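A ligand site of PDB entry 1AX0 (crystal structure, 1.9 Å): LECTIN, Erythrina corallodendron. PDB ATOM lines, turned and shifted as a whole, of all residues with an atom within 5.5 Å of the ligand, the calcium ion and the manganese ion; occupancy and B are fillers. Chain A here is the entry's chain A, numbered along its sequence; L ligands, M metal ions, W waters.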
ATOM      1  N   LEU A  86     -16.508  -7.633 -24.348  1.00  0.00           N
ATOM      2  CA  LEU A  86     -16.633  -7.327 -25.776  1.00  0.00           C
ATOM      3  C   LEU A  86     -15.547  -6.342 -26.210  1.00  0.00           C
ATOM      4  O   LEU A  86     -15.239  -5.383 -25.501  1.00  0.00           O
ATOM      5  CB  LEU A  86     -18.012  -6.710 -26.061  1.00  0.00           C
ATOM      6  CG  LEU A  86     -19.245  -7.563 -25.715  1.00  0.00           C
ATOM      7  CD1 LEU A  86     -20.506  -6.727 -25.887  1.00  0.00           C
ATOM      8  CD2 LEU A  86     -19.296  -8.802 -26.587  1.00  0.00           C
ATOM      9  N   ALA A  88     -13.525  -3.337 -28.309  1.00  0.00           N
ATOM     10  CA  ALA A  88     -13.904  -1.955 -28.619  1.00  0.00           C
ATOM     11  C   ALA A  88     -12.635  -1.175 -28.948  1.00  0.00           C
ATOM     12  O   ALA A  88     -11.539  -1.656 -28.629  1.00  0.00           O
ATOM     13  CB  ALA A  88     -14.598  -1.342 -27.406  1.00  0.00           C
ATOM     14  N   ASP A  89     -12.730   0.000 -29.594  1.00  0.00           N
ATOM     15  CA  ASP A  89     -13.972   0.638 -30.034  1.00  0.00           C
ATOM     16  C   ASP A  89     -14.027   0.801 -31.560  1.00  0.00           C
ATOM     17  O   ASP A  89     -15.111   0.899 -32.141  1.00  0.00           O
ATOM     18  CB  ASP A  89     -14.118   2.022 -29.400  1.00  0.00           C
ATOM     19  CG  ASP A  89     -14.880   1.995 -28.097  1.00  0.00           C
ATOM     20  OD1 ASP A  89     -16.125   1.851 -28.128  1.00  0.00           O
ATOM     21  OD2 ASP A  89     -14.230   2.098 -27.035  1.00  0.00           O
ATOM     22  N   GLY A 105     -11.989   9.685 -26.337  1.00  0.00           N
ATOM     23  CA  GLY A 105     -11.723   8.367 -26.867  1.00  0.00           C
ATOM     24  C   GLY A 105     -12.941   7.467 -26.789  1.00  0.00           C
ATOM     25  O   GLY A 105     -14.085   7.926 -26.898  1.00  0.00           O
ATOM     26  N   TYR A 106     -12.692   6.179 -26.573  1.00  0.00           N
ATOM     27  CA  TYR A 106     -13.751   5.165 -26.471  1.00  0.00           C
ATOM     28  C   TYR A 106     -14.678   5.213 -27.684  1.00  0.00           C
ATOM     29  O   TYR A 106     -14.203   5.330 -28.827  1.00  0.00           O
ATOM     30  CB  TYR A 106     -14.554   5.349 -25.172  1.00  0.00           C
ATOM     31  CG  TYR A 106     -13.689   5.560 -23.949  1.00  0.00           C
ATOM     32  CD1 TYR A 106     -12.554   4.781 -23.724  1.00  0.00           C
ATOM     33  CD2 TYR A 106     -13.992   6.556 -23.028  1.00  0.00           C
ATOM     34  CE1 TYR A 106     -11.738   4.994 -22.619  1.00  0.00           C
ATOM     35  CE2 TYR A 106     -13.182   6.779 -21.914  1.00  0.00           C
ATOM     36  CZ  TYR A 106     -12.055   6.003 -21.720  1.00  0.00           C
ATOM     37  OH  TYR A 106     -11.247   6.222 -20.635  1.00  0.00           O
ATOM     38  N   GLY A 107     -15.983   5.157 -27.450  1.00  0.00           N
ATOM     39  CA  GLY A 107     -16.956   5.178 -28.535  1.00  0.00           C
ATOM     40  C   GLY A 107     -16.940   6.425 -29.401  1.00  0.00           C
ATOM     41  O   GLY A 107     -17.531   6.421 -30.481  1.00  0.00           O
ATOM     42  N   TYR A 108     -16.292   7.485 -28.934  1.00  0.00           N
ATOM     43  CA  TYR A 108     -16.207   8.733 -29.694  1.00  0.00           C
ATOM     44  C   TYR A 108     -15.071   8.697 -30.703  1.00  0.00           C
ATOM     45  O   TYR A 108     -14.895   9.630 -31.489  1.00  0.00           O
ATOM     46  CB  TYR A 108     -16.100   9.931 -28.760  1.00  0.00           C
ATOM     47  CG  TYR A 108     -17.271   9.999 -27.804  1.00  0.00           C
ATOM     48  CD1 TYR A 108     -18.555  10.227 -28.277  1.00  0.00           C
ATOM     49  CD2 TYR A 108     -17.089   9.785 -26.443  1.00  0.00           C
ATOM     50  CE1 TYR A 108     -19.639  10.228 -27.419  1.00  0.00           C
ATOM     51  CE2 TYR A 108     -18.171   9.788 -25.565  1.00  0.00           C
ATOM     52  CZ  TYR A 108     -19.451  10.006 -26.057  1.00  0.00           C
ATOM     53  OH  TYR A 108     -20.528  10.012 -25.211  1.00  0.00           O
ATOM     54  N   GLU A 127     -16.191   5.597 -40.372  1.00  0.00           N
ATOM     55  CA  GLU A 127     -15.786   4.732 -39.283  1.00  0.00           C
ATOM     56  C   GLU A 127     -15.944   3.247 -39.538  1.00  0.00           C
ATOM     57  O   GLU A 127     -16.740   2.813 -40.362  1.00  0.00           O
ATOM     58  CB  GLU A 127     -16.602   5.081 -38.047  1.00  0.00           C
ATOM     59  CG  GLU A 127     -18.091   4.916 -38.310  1.00  0.00           C
ATOM     60  CD  GLU A 127     -18.914   4.950 -37.071  1.00  0.00           C
ATOM     61  OE1 GLU A 127     -18.823   5.905 -36.296  1.00  0.00           O
ATOM     62  OE2 GLU A 127     -19.671   3.979 -36.895  1.00  0.00           O
ATOM     63  N   ASP A 129     -16.540   0.713 -36.898  1.00  0.00           N
ATOM     64  CA  ASP A 129     -16.960   0.581 -35.514  1.00  0.00           C
ATOM     65  C   ASP A 129     -17.149  -0.860 -35.034  1.00  0.00           C
ATOM     66  O   ASP A 129     -17.969  -1.588 -35.564  1.00  0.00           O
ATOM     67  CB  ASP A 129     -18.262   1.343 -35.380  1.00  0.00           C
ATOM     68  CG  ASP A 129     -18.614   1.668 -33.961  1.00  0.00           C
ATOM     69  OD1 ASP A 129     -18.113   1.023 -33.021  1.00  0.00           O
ATOM     70  OD2 ASP A 129     -19.410   2.596 -33.795  1.00  0.00           O
ATOM     71  N   THR A 130     -16.468  -1.194 -33.936  1.00  0.00           N
ATOM     72  CA  THR A 130     -16.499  -2.542 -33.388  1.00  0.00           C
ATOM     73  C   THR A 130     -17.319  -2.746 -32.107  1.00  0.00           C
ATOM     74  O   THR A 130     -17.480  -3.884 -31.649  1.00  0.00           O
ATOM     75  CB  THR A 130     -15.067  -3.041 -33.143  1.00  0.00           C
ATOM     76  OG1 THR A 130     -14.391  -2.133 -32.262  1.00  0.00           O
ATOM     77  CG2 THR A 130     -14.304  -3.129 -34.451  1.00  0.00           C
ATOM     78  N   PHE A 131     -17.847  -1.674 -31.535  1.00  0.00           N
ATOM     79  CA  PHE A 131     -18.631  -1.790 -30.309  1.00  0.00           C
ATOM     80  C   PHE A 131     -19.957  -1.042 -30.444  1.00  0.00           C
ATOM     81  O   PHE A 131     -19.970   0.100 -30.859  1.00  0.00           O
ATOM     82  CB  PHE A 131     -17.835  -1.238 -29.116  1.00  0.00           C
ATOM     83  CG  PHE A 131     -18.563  -1.340 -27.805  1.00  0.00           C
ATOM     84  CD1 PHE A 131     -18.427  -2.471 -27.015  1.00  0.00           C
ATOM     85  CD2 PHE A 131     -19.395  -0.306 -27.367  1.00  0.00           C
ATOM     86  CE1 PHE A 131     -19.126  -2.583 -25.806  1.00  0.00           C
ATOM     87  CE2 PHE A 131     -20.094  -0.405 -26.169  1.00  0.00           C
ATOM     88  CZ  PHE A 131     -19.959  -1.550 -25.378  1.00  0.00           C
ATOM     89  N   SER A 132     -21.049  -1.687 -30.045  1.00  0.00           N
ATOM     90  CA  SER A 132     -22.358  -1.053 -30.156  1.00  0.00           C
ATOM     91  C   SER A 132     -22.730  -0.168 -28.963  1.00  0.00           C
ATOM     92  O   SER A 132     -23.076  -0.677 -27.898  1.00  0.00           O
ATOM     93  CB  SER A 132     -23.443  -2.125 -30.378  1.00  0.00           C
ATOM     94  OG  SER A 132     -24.682  -1.515 -30.713  1.00  0.00           O
ATOM     95  N   ASN A 133     -22.618   1.142 -29.157  1.00  0.00           N
ATOM     96  CA  ASN A 133     -22.973   2.131 -28.131  1.00  0.00           C
ATOM     97  C   ASN A 133     -24.482   2.386 -28.227  1.00  0.00           C
ATOM     98  O   ASN A 133     -25.133   1.894 -29.145  1.00  0.00           O
ATOM     99  CB  ASN A 133     -22.187   3.430 -28.353  1.00  0.00           C
ATOM    100  CG  ASN A 133     -20.701   3.252 -28.184  1.00  0.00           C
ATOM    101  OD1 ASN A 133     -19.981   3.052 -29.151  1.00  0.00           O
ATOM    102  ND2 ASN A 133     -20.221   3.333 -26.946  1.00  0.00           N
ATOM    103  N   TRP A 135     -26.080   4.837 -29.320  1.00  0.00           N
ATOM    104  CA  TRP A 135     -26.411   5.558 -30.556  1.00  0.00           C
ATOM    105  C   TRP A 135     -26.158   4.728 -31.808  1.00  0.00           C
ATOM    106  O   TRP A 135     -26.420   5.178 -32.932  1.00  0.00           O
ATOM    107  CB  TRP A 135     -25.582   6.851 -30.638  1.00  0.00           C
ATOM    108  CG  TRP A 135     -24.093   6.617 -30.554  1.00  0.00           C
ATOM    109  CD1 TRP A 135     -23.278   6.144 -31.551  1.00  0.00           C
ATOM    110  CD2 TRP A 135     -23.252   6.853 -29.423  1.00  0.00           C
ATOM    111  NE1 TRP A 135     -21.983   6.077 -31.101  1.00  0.00           N
ATOM    112  CE2 TRP A 135     -21.931   6.501 -29.796  1.00  0.00           C
ATOM    113  CE3 TRP A 135     -23.487   7.315 -28.122  1.00  0.00           C
ATOM    114  CZ2 TRP A 135     -20.855   6.611 -28.918  1.00  0.00           C
ATOM    115  CZ3 TRP A 135     -22.398   7.424 -27.245  1.00  0.00           C
ATOM    116  CH2 TRP A 135     -21.100   7.075 -27.657  1.00  0.00           C
ATOM    117  N   ASP A 136     -25.637   3.515 -31.612  1.00  0.00           N
ATOM    118  CA  ASP A 136     -25.314   2.600 -32.707  1.00  0.00           C
ATOM    119  C   ASP A 136     -26.371   1.568 -33.027  1.00  0.00           C
ATOM    120  O   ASP A 136     -27.241   1.277 -32.196  1.00  0.00           O
ATOM    121  CB  ASP A 136     -24.068   1.780 -32.333  1.00  0.00           C
ATOM    122  CG  ASP A 136     -22.807   2.570 -32.441  1.00  0.00           C
ATOM    123  OD1 ASP A 136     -22.738   3.421 -33.329  1.00  0.00           O
ATOM    124  OD2 ASP A 136     -21.893   2.365 -31.630  1.00  0.00           O
ATOM    125  N   PRO A 137     -26.332   1.031 -34.253  1.00  0.00           N
ATOM    126  CA  PRO A 137     -27.299   0.005 -34.621  1.00  0.00           C
ATOM    127  C   PRO A 137     -26.766  -1.207 -33.849  1.00  0.00           C
ATOM    128  O   PRO A 137     -25.591  -1.232 -33.446  1.00  0.00           O
ATOM    129  CB  PRO A 137     -27.089  -0.145 -36.123  1.00  0.00           C
ATOM    130  CG  PRO A 137     -25.651   0.240 -36.321  1.00  0.00           C
ATOM    131  CD  PRO A 137     -25.532   1.446 -35.429  1.00  0.00           C
ATOM    132  N   HIS A 142     -19.466  -2.402 -38.026  1.00  0.00           N
ATOM    133  CA  HIS A 142     -20.161  -1.758 -39.124  1.00  0.00           C
ATOM    134  C   HIS A 142     -19.383  -0.564 -39.634  1.00  0.00           C
ATOM    135  O   HIS A 142     -18.563   0.010 -38.922  1.00  0.00           O
ATOM    136  CB  HIS A 142     -21.588  -1.349 -38.731  1.00  0.00           C
ATOM    137  CG  HIS A 142     -21.664  -0.432 -37.543  1.00  0.00           C
ATOM    138  ND1 HIS A 142     -22.010  -0.847 -36.279  1.00  0.00           N
ATOM    139  CD2 HIS A 142     -21.427   0.899 -37.446  1.00  0.00           C
ATOM    140  CE1 HIS A 142     -21.968   0.225 -35.475  1.00  0.00           C
ATOM    141  NE2 HIS A 142     -21.618   1.306 -36.141  1.00  0.00           N
ATOM    142  N   ILE A 150     -21.242  11.352 -34.109  1.00  0.00           N
ATOM    143  CA  ILE A 150     -20.855   9.948 -33.989  1.00  0.00           C
ATOM    144  C   ILE A 150     -22.075   9.089 -34.382  1.00  0.00           C
ATOM    145  O   ILE A 150     -21.949   7.886 -34.614  1.00  0.00           O
ATOM    146  CB  ILE A 150     -20.373   9.636 -32.536  1.00  0.00           C
ATOM    147  CG1 ILE A 150     -19.700   8.266 -32.472  1.00  0.00           C
ATOM    148  CG2 ILE A 150     -21.525   9.785 -31.551  1.00  0.00           C
ATOM    149  CD1 ILE A 150     -18.400   8.187 -33.264  1.00  0.00           C
ATOM    150  N   SER A 152     -24.028   7.986 -36.994  1.00  0.00           N
ATOM    151  CA  SER A 152     -23.922   7.897 -38.447  1.00  0.00           C
ATOM    152  C   SER A 152     -25.206   8.154 -39.227  1.00  0.00           C
ATOM    153  O   SER A 152     -26.289   7.763 -38.802  1.00  0.00           O
ATOM    154  CB  SER A 152     -23.384   6.525 -38.858  1.00  0.00           C
ATOM    155  OG  SER A 152     -22.210   6.201 -38.131  1.00  0.00           O
ATOM    156  N   THR A 216      -9.449   2.220 -28.079  1.00  0.00           N
ATOM    157  CA  THR A 216      -9.821   0.995 -27.381  1.00  0.00           C
ATOM    158  C   THR A 216     -10.782   1.372 -26.259  1.00  0.00           C
ATOM    159  O   THR A 216     -10.935   2.548 -25.930  1.00  0.00           O
ATOM    160  CB  THR A 216      -8.599   0.206 -26.858  1.00  0.00           C
ATOM    161  OG1 THR A 216      -7.750   1.064 -26.095  1.00  0.00           O
ATOM    162  CG2 THR A 216      -7.829  -0.393 -28.018  1.00  0.00           C
ATOM    163  N   GLY A 217     -11.414   0.354 -25.661  1.00  0.00           N
ATOM    164  CA  GLY A 217     -12.424   0.544 -24.632  1.00  0.00           C
ATOM    165  C   GLY A 217     -12.180   1.178 -23.268  1.00  0.00           C
ATOM    166  O   GLY A 217     -11.047   1.316 -22.813  1.00  0.00           O
ATOM    167  N   ALA A 218     -13.282   1.485 -22.601  1.00  0.00           N
ATOM    168  CA  ALA A 218     -13.297   2.125 -21.290  1.00  0.00           C
ATOM    169  C   ALA A 218     -13.152   1.174 -20.091  1.00  0.00           C
ATOM    170  O   ALA A 218     -13.055   1.634 -18.956  1.00  0.00           O
ATOM    171  CB  ALA A 218     -14.553   2.965 -21.129  1.00  0.00           C
ATOM    172  N   GLN A 219     -13.181  -0.129 -20.338  1.00  0.00           N
ATOM    173  CA  GLN A 219     -13.009  -1.092 -19.250  1.00  0.00           C
ATOM    174  C   GLN A 219     -11.884  -2.062 -19.566  1.00  0.00           C
ATOM    175  O   GLN A 219     -11.516  -2.251 -20.721  1.00  0.00           O
ATOM    176  CB  GLN A 219     -14.318  -1.843 -18.953  1.00  0.00           C
ATOM    177  CG  GLN A 219     -14.816  -2.764 -20.047  1.00  0.00           C
ATOM    178  CD  GLN A 219     -16.004  -3.599 -19.585  1.00  0.00           C
ATOM    179  OE1 GLN A 219     -15.835  -4.622 -18.924  1.00  0.00           O
ATOM    180  NE2 GLN A 219     -17.209  -3.168 -19.939  1.00  0.00           N
ATOM    181  N   ALA A 222     -11.207  -4.475 -22.792  1.00  0.00           N
ATOM    182  CA  ALA A 222     -12.187  -4.225 -23.846  1.00  0.00           C
ATOM    183  C   ALA A 222     -11.288  -3.525 -24.866  1.00  0.00           C
ATOM    184  O   ALA A 222     -11.244  -2.299 -24.943  1.00  0.00           O
ATOM    185  CB  ALA A 222     -13.277  -3.279 -23.368  1.00  0.00           C
HETATM  186  O1  LIG L   1     -17.197   1.029 -22.436  1.00  0.00           O
HETATM  187  C1  LIG L   1     -18.154   2.092 -22.499  1.00  0.00           C
HETATM  188  O2  LIG L   1     -19.410   1.522 -22.604  1.00  0.00           O
HETATM  189  C2  LIG L   1     -17.894   2.983 -23.720  1.00  0.00           C
HETATM  190  N1  LIG L   1     -18.964   3.964 -23.834  1.00  0.00           N
HETATM  191  C3  LIG L   1     -17.829   2.153 -25.009  1.00  0.00           C
HETATM  192  O3  LIG L   1     -17.446   2.984 -26.100  1.00  0.00           O
HETATM  193  C4  LIG L   1     -16.830   1.015 -24.838  1.00  0.00           C
HETATM  194  O4  LIG L   1     -15.525   1.554 -24.662  1.00  0.00           O
HETATM  195  C5  LIG L   1     -17.219   0.189 -23.617  1.00  0.00           C
HETATM  196  C6  LIG L   1     -16.274  -0.960 -23.359  1.00  0.00           C
HETATM  197  O5  LIG L   1     -16.807  -1.859 -22.400  1.00  0.00           O
HETATM  198  C7  LIG L   1     -18.681   5.258 -23.867  1.00  0.00           C
HETATM  199  O6  LIG L   1     -17.543   5.705 -23.808  1.00  0.00           O
HETATM  200  C8  LIG L   1     -19.861   6.214 -23.990  1.00  0.00           C
HETATM  201 CA    CA M   1     -19.483   2.371 -31.392  1.00  0.00          CA
HETATM  202 MN    MN M   2     -21.169   3.458 -35.118  1.00  0.00          MN
HETATM  203  O   HOH W   1     -19.962   1.388 -19.672  1.00  0.00           O
HETATM  204  O   HOH W   2     -17.201   2.202 -30.555  1.00  0.00           O
HETATM  205  O   HOH W   3     -20.536   5.669 -34.247  1.00  0.00           O
HETATM  206  O   HOH W   4     -16.791  -4.346 -23.463  1.00  0.00           O
HETATM  207  O   HOH W   5     -21.724   3.342 -24.581  1.00  0.00           O
HETATM  208  O   HOH W   6     -17.011   8.163 -22.336  1.00  0.00           O
HETATM  209  O   HOH W   7     -19.210   4.761 -31.804  1.00  0.00           O
HETATM  210  O   HOH W   8     -23.035   4.311 -36.431  1.00  0.00           O
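The nearest printed residue that does not touch the calcium ion is Trp 135 (4.5 Å).
OD1 of Asp 89 is in hydrogen-bond range of N of Gly 107, 3.4 Å away.
The backbone NH of Thr 130 is in hydrogen-bond range of the backbone carbonyl oxygen of Asp 89, 3.1 Å away.
The backbone NH of Gly 217 is in hydrogen-bond range of the backbone carbonyl oxygen of Ala 222, at 2.8 Å.
Merely in contact with the ligand: Gly 217 (3.3 Å), Tyr 106 (3.3 Å), Ala 222 (3.8 Å) and Trp 135 (3.97 Å).
Hydrophobic or aromatic side chains within 4 Å of the ligand: Tyr 106, Phe 131, Trp 135, Ala 218 and Ala 222.
Of the 24 residues printed, 10 come within 4 Å of the ligand.
The nearest printed residue that does not touch the ligand is Tyr 108 (4.04 Å).
The calcium ion is bound by the backbone carbonyl oxygen (O) of Phe 131, the side-chain amide oxygen (OD1) of Asn 133, the side-chain carboxylate (OD2) of Asp 129, the side-chain carboxylate (OD2) of Asp 136, water W2, water W7 and the side-chain carboxylate (OD1) of Asp 129.
The calcium ion has seven donor atoms within binding distance.
Water W7 bridges O of Gly 107 (2.7 Å) and NE1 of Trp 135 (3.1 Å).
Water W3 lies within hydrogen-bond range of O of Ile 150 (2.7 Å), OE1 of Glu 127 (2.7 Å) and NE1 of Trp 135 (3.5 Å).
Water W4 lies within hydrogen-bond range of an oxygen (O5) of the ligand and the backbone carbonyl oxygen of Leu 86.
Water W5 bridges ND2 of Asn 133 (2.8 Å) and N1 of the ligand (2.9 Å).
O3 of the ligand lies within hydrogen-bond range of ND2 of Asn 133 (2.9 Å).
The side-chain carboxylate (OD1) of Asp 89 is in hydrogen-bond range of an oxygen (O3) of the ligand, 2.7 Å away.
The side-chain amide nitrogen (NE2) of Gln 219 is in hydrogen-bond range of an oxygen (O5) of the ligand (2.8 Å).
The backbone NH (N) of Gly 107 sits at hydrogen-bond distance from an oxygen (O3) of the ligand.
The backbone NH of Ala 218 is in hydrogen-bond range of an oxygen (O4) of the ligand (3.0 Å).
The manganese ion is bound by the side-chain carboxylate of Asp 129 (2.4 Å), the side-chain carboxylate of Asp 136 (2.4 Å), the side-chain carboxylate of Glu 127 (2.4 Å), a ring nitrogen (NE2) of His 142 (2.4 Å), water W8 (2.4 Å) and water W3 (2.5 Å).
The manganese ion has six donor atoms within binding distance.
Within 4 Å of the manganese ion: Glu 127, Asp 129, Asp 136 and His 142.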
